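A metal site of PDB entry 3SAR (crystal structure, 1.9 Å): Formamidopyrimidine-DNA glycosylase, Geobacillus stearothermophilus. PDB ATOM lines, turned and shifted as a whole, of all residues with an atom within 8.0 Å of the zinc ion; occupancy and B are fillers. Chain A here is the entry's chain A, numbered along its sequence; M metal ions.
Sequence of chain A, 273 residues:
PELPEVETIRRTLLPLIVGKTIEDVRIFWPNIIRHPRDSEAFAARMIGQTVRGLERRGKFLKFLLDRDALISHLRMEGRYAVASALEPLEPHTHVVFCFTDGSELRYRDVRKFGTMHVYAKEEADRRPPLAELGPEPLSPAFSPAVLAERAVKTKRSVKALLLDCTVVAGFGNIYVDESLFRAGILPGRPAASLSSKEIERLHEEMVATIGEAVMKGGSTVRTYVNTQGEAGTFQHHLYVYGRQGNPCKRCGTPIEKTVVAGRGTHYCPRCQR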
ATOM      1  N   PHE A 181      15.477 -26.748  24.679  1.00  0.00           N
ATOM      2  CA  PHE A 181      15.723 -27.131  23.301  1.00  0.00           C
ATOM      3  C   PHE A 181      17.000 -27.964  23.188  1.00  0.00           C
ATOM      4  O   PHE A 181      17.036 -28.995  22.528  1.00  0.00           O
ATOM      5  CB  PHE A 181      15.843 -25.929  22.377  1.00  0.00           C
ATOM      6  CG  PHE A 181      16.436 -26.289  21.044  1.00  0.00           C
ATOM      7  CD1 PHE A 181      15.637 -26.869  20.055  1.00  0.00           C
ATOM      8  CD2 PHE A 181      17.780 -26.130  20.800  1.00  0.00           C
ATOM      9  CE1 PHE A 181      16.172 -27.233  18.844  1.00  0.00           C
ATOM     10  CE2 PHE A 181      18.334 -26.484  19.585  1.00  0.00           C
ATOM     11  CZ  PHE A 181      17.534 -27.042  18.597  1.00  0.00           C
ATOM     12  N   TYR A 239      18.771 -20.612  19.615  1.00  0.00           N
ATOM     13  CA  TYR A 239      18.191 -21.706  18.847  1.00  0.00           C
ATOM     14  C   TYR A 239      16.704 -21.547  18.626  1.00  0.00           C
ATOM     15  O   TYR A 239      16.197 -21.838  17.536  1.00  0.00           O
ATOM     16  CB  TYR A 239      18.450 -23.042  19.545  1.00  0.00           C
ATOM     17  CG  TYR A 239      19.883 -23.516  19.468  1.00  0.00           C
ATOM     18  CD1 TYR A 239      20.696 -23.505  20.584  1.00  0.00           C
ATOM     19  CD2 TYR A 239      20.421 -23.960  18.257  1.00  0.00           C
ATOM     20  CE1 TYR A 239      22.009 -23.934  20.522  1.00  0.00           C
ATOM     21  CE2 TYR A 239      21.734 -24.384  18.183  1.00  0.00           C
ATOM     22  CZ  TYR A 239      22.526 -24.367  19.317  1.00  0.00           C
ATOM     23  OH  TYR A 239      23.822 -24.793  19.257  1.00  0.00           O
ATOM     24  N   VAL A 240      15.984 -21.118  19.666  1.00  0.00           N
ATOM     25  CA  VAL A 240      14.523 -21.081  19.603  1.00  0.00           C
ATOM     26  C   VAL A 240      13.898 -19.761  20.065  1.00  0.00           C
ATOM     27  O   VAL A 240      12.881 -19.332  19.523  1.00  0.00           O
ATOM     28  CB  VAL A 240      13.873 -22.252  20.404  1.00  0.00           C
ATOM     29  CG1 VAL A 240      14.166 -23.606  19.733  1.00  0.00           C
ATOM     30  CG2 VAL A 240      14.332 -22.252  21.849  1.00  0.00           C
ATOM     31  N   PRO A 247      13.424 -21.436  10.543  1.00  0.00           N
ATOM     32  CA  PRO A 247      13.843 -22.840  10.589  1.00  0.00           C
ATOM     33  C   PRO A 247      14.738 -23.127  11.786  1.00  0.00           C
ATOM     34  O   PRO A 247      15.589 -22.316  12.133  1.00  0.00           O
ATOM     35  CB  PRO A 247      14.646 -23.006   9.273  1.00  0.00           C
ATOM     36  CG  PRO A 247      14.978 -21.593   8.857  1.00  0.00           C
ATOM     37  CD  PRO A 247      13.776 -20.815   9.256  1.00  0.00           C
ATOM     38  N   CYS A 248      14.526 -24.282  12.398  1.00  0.00           N
ATOM     39  CA  CYS A 248      15.402 -24.767  13.454  1.00  0.00           C
ATOM     40  C   CYS A 248      16.829 -24.937  12.925  1.00  0.00           C
ATOM     41  O   CYS A 248      17.048 -25.440  11.820  1.00  0.00           O
ATOM     42  CB  CYS A 248      14.873 -26.091  14.011  1.00  0.00           C
ATOM     43  SG  CYS A 248      16.010 -26.964  15.136  1.00  0.00           S
ATOM     44  N   LYS A 249      17.802 -24.508  13.729  1.00  0.00           N
ATOM     45  CA  LYS A 249      19.192 -24.510  13.325  1.00  0.00           C
ATOM     46  C   LYS A 249      19.776 -25.911  13.258  1.00  0.00           C
ATOM     47  O   LYS A 249      20.793 -26.136  12.606  1.00  0.00           O
ATOM     48  CB  LYS A 249      20.015 -23.622  14.269  1.00  0.00           C
ATOM     49  CG  LYS A 249      19.650 -22.150  14.171  1.00  0.00           C
ATOM     50  CD  LYS A 249      20.640 -21.265  14.933  1.00  0.00           C
ATOM     51  CE  LYS A 249      20.212 -19.804  14.880  1.00  0.00           C
ATOM     52  NZ  LYS A 249      21.120 -18.930  15.664  1.00  0.00           N
ATOM     53  N   ARG A 250      19.115 -26.867  13.913  1.00  0.00           N
ATOM     54  CA  ARG A 250      19.595 -28.244  13.874  1.00  0.00           C
ATOM     55  C   ARG A 250      18.855 -29.180  12.908  1.00  0.00           C
ATOM     56  O   ARG A 250      19.464 -30.108  12.382  1.00  0.00           O
ATOM     57  CB  ARG A 250      19.618 -28.857  15.276  1.00  0.00           C
ATOM     58  CG  ARG A 250      20.668 -28.170  16.165  1.00  0.00           C
ATOM     59  CD  ARG A 250      20.910 -28.911  17.464  1.00  0.00           C
ATOM     60  NE  ARG A 250      21.915 -28.225  18.272  1.00  0.00           N
ATOM     61  CZ  ARG A 250      22.122 -28.452  19.560  1.00  0.00           C
ATOM     62  NH1 ARG A 250      23.061 -27.768  20.212  1.00  0.00           N
ATOM     63  NH2 ARG A 250      21.394 -29.354  20.208  1.00  0.00           N
ATOM     64  N   CYS A 251      17.558 -28.959  12.687  1.00  0.00           N
ATOM     65  CA  CYS A 251      16.800 -29.849  11.792  1.00  0.00           C
ATOM     66  C   CYS A 251      16.017 -29.149  10.684  1.00  0.00           C
ATOM     67  O   CYS A 251      15.482 -29.799   9.793  1.00  0.00           O
ATOM     68  CB  CYS A 251      15.853 -30.746  12.588  1.00  0.00           C
ATOM     69  SG  CYS A 251      14.401 -29.863  13.203  1.00  0.00           S
ATOM     70  N   GLY A 252      15.939 -27.820  10.746  1.00  0.00           N
ATOM     71  CA  GLY A 252      15.267 -27.070   9.698  1.00  0.00           C
ATOM     72  C   GLY A 252      13.758 -26.954   9.855  1.00  0.00           C
ATOM     73  O   GLY A 252      13.104 -26.232   9.104  1.00  0.00           O
ATOM     74  N   THR A 253      13.196 -27.673  10.821  1.00  0.00           N
ATOM     75  CA  THR A 253      11.772 -27.549  11.143  1.00  0.00           C
ATOM     76  C   THR A 253      11.443 -26.138  11.656  1.00  0.00           C
ATOM     77  O   THR A 253      12.207 -25.548  12.431  1.00  0.00           O
ATOM     78  CB  THR A 253      11.356 -28.588  12.202  1.00  0.00           C
ATOM     79  OG1 THR A 253      11.686 -29.902  11.741  1.00  0.00           O
ATOM     80  CG2 THR A 253       9.844 -28.500  12.485  1.00  0.00           C
ATOM     81  N   PRO A 254      10.292 -25.585  11.235  1.00  0.00           N
ATOM     82  CA  PRO A 254       9.971 -24.245  11.728  1.00  0.00           C
ATOM     83  C   PRO A 254       9.769 -24.209  13.239  1.00  0.00           C
ATOM     84  O   PRO A 254       9.061 -25.039  13.785  1.00  0.00           O
ATOM     85  CB  PRO A 254       8.663 -23.902  11.009  1.00  0.00           C
ATOM     86  CG  PRO A 254       8.675 -24.765   9.779  1.00  0.00           C
ATOM     87  CD  PRO A 254       9.357 -26.043  10.192  1.00  0.00           C
ATOM     88  N   ILE A 255      10.418 -23.250  13.893  1.00  0.00           N
ATOM     89  CA  ILE A 255      10.239 -23.044  15.324  1.00  0.00           C
ATOM     90  C   ILE A 255       8.807 -22.586  15.590  1.00  0.00           C
ATOM     91  O   ILE A 255       8.235 -21.799  14.830  1.00  0.00           O
ATOM     92  CB  ILE A 255      11.241 -22.015  15.852  1.00  0.00           C
ATOM     93  CG1 ILE A 255      12.664 -22.553  15.691  1.00  0.00           C
ATOM     94  CG2 ILE A 255      10.950 -21.674  17.315  1.00  0.00           C
ATOM     95  CD1 ILE A 255      12.795 -24.015  16.144  1.00  0.00           C
ATOM     96  N   TYR A 267       9.880 -23.407  20.856  1.00  0.00           N
ATOM     97  CA  TYR A 267      10.411 -24.758  20.811  1.00  0.00           C
ATOM     98  C   TYR A 267      10.409 -25.327  19.381  1.00  0.00           C
ATOM     99  O   TYR A 267       9.692 -24.829  18.505  1.00  0.00           O
ATOM    100  CB  TYR A 267       9.599 -25.676  21.728  1.00  0.00           C
ATOM    101  CG  TYR A 267       8.156 -25.819  21.257  1.00  0.00           C
ATOM    102  CD1 TYR A 267       7.808 -26.829  20.366  1.00  0.00           C
ATOM    103  CD2 TYR A 267       7.166 -24.946  21.689  1.00  0.00           C
ATOM    104  CE1 TYR A 267       6.496 -26.964  19.937  1.00  0.00           C
ATOM    105  CE2 TYR A 267       5.854 -25.082  21.260  1.00  0.00           C
ATOM    106  CZ  TYR A 267       5.529 -26.094  20.374  1.00  0.00           C
ATOM    107  OH  TYR A 267       4.231 -26.242  19.933  1.00  0.00           O
ATOM    108  N   CYS A 268      11.215 -26.370  19.166  1.00  0.00           N
ATOM    109  CA  CYS A 268      11.170 -27.124  17.919  1.00  0.00           C
ATOM    110  C   CYS A 268      10.404 -28.420  18.134  1.00  0.00           C
ATOM    111  O   CYS A 268      10.786 -29.233  18.976  1.00  0.00           O
ATOM    112  CB  CYS A 268      12.590 -27.439  17.427  1.00  0.00           C
ATOM    113  SG  CYS A 268      12.578 -28.573  15.968  1.00  0.00           S
ATOM    114  N   PRO A 269       9.323 -28.634  17.370  1.00  0.00           N
ATOM    115  CA  PRO A 269       8.482 -29.799  17.638  1.00  0.00           C
ATOM    116  C   PRO A 269       9.145 -31.098  17.167  1.00  0.00           C
ATOM    117  O   PRO A 269       8.595 -32.166  17.435  1.00  0.00           O
ATOM    118  CB  PRO A 269       7.226 -29.516  16.804  1.00  0.00           C
ATOM    119  CG  PRO A 269       7.748 -28.655  15.666  1.00  0.00           C
ATOM    120  CD  PRO A 269       8.728 -27.745  16.355  1.00  0.00           C
ATOM    121  N   ARG A 270      10.272 -31.000  16.472  1.00  0.00           N
ATOM    122  CA  ARG A 270      10.966 -32.212  16.025  1.00  0.00           C
ATOM    123  C   ARG A 270      12.108 -32.566  16.967  1.00  0.00           C
ATOM    124  O   ARG A 270      12.201 -33.694  17.417  1.00  0.00           O
ATOM    125  CB  ARG A 270      11.481 -32.076  14.587  1.00  0.00           C
ATOM    126  CG  ARG A 270      12.184 -33.340  14.105  1.00  0.00           C
ATOM    127  CD  ARG A 270      12.642 -33.247  12.653  1.00  0.00           C
ATOM    128  NE  ARG A 270      13.214 -34.523  12.225  1.00  0.00           N
ATOM    129  CZ  ARG A 270      13.545 -34.810  10.969  1.00  0.00           C
ATOM    130  NH1 ARG A 270      14.063 -35.992  10.685  1.00  0.00           N
ATOM    131  NH2 ARG A 270      13.364 -33.893  10.005  1.00  0.00           N
ATOM    132  N   CYS A 271      12.967 -31.597  17.275  1.00  0.00           N
ATOM    133  CA  CYS A 271      14.075 -31.858  18.177  1.00  0.00           C
ATOM    134  C   CYS A 271      13.648 -32.149  19.607  1.00  0.00           C
ATOM    135  O   CYS A 271      14.299 -32.924  20.307  1.00  0.00           O
ATOM    136  CB  CYS A 271      15.098 -30.698  18.164  1.00  0.00           C
ATOM    137  SG  CYS A 271      16.023 -30.573  16.604  1.00  0.00           S
ATOM    138  N   GLN A 272      12.562 -31.517  20.066  1.00  0.00           N
ATOM    139  CA  GLN A 272      12.146 -31.694  21.455  1.00  0.00           C
ATOM    140  C   GLN A 272      10.971 -32.657  21.564  1.00  0.00           C
ATOM    141  O   GLN A 272      10.061 -32.636  20.729  1.00  0.00           O
ATOM    142  CB  GLN A 272      11.810 -30.338  22.098  1.00  0.00           C
ATOM    143  CG  GLN A 272      12.983 -29.362  22.100  1.00  0.00           C
ATOM    144  CD  GLN A 272      12.589 -27.936  22.440  1.00  0.00           C
ATOM    145  OE1 GLN A 272      12.626 -27.052  21.574  1.00  0.00           O
ATOM    146  NE2 GLN A 272      12.231 -27.695  23.694  1.00  0.00           N
HETATM  147 ZN    ZN M   1      14.812 -28.988  15.363  1.00  0.00          ZN
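The zinc ion is bound by the side-chain sulfur of Cys 271 (2.3 Å), the side-chain sulfur of Cys 268 (2.4 Å), the side-chain sulfur of Cys 248 (2.4 Å) and the side-chain sulfur of Cys 251 (2.4 Å).
The zinc ion has four donor atoms within binding distance.
The side-chain sulfur of Cys 268 lies close to the backbone NH of Arg 270, at 3.4 Å.
The backbone NH (N) of Cys 268 sits at hydrogen-bond distance from the side-chain amide oxygen (OE1) of Gln 272 (2.9 Å).
The backbone carbonyl oxygen of Thr 253 sits at hydrogen-bond distance from the backbone NH of Cys 248 (2.6 Å).
SG of Cys 248 sits close to N of Arg 250 (3.3 Å).
The side-chain sulfur of Cys 251 sits close to the side-chain hydroxyl of Thr 253, 3.1 Å away.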
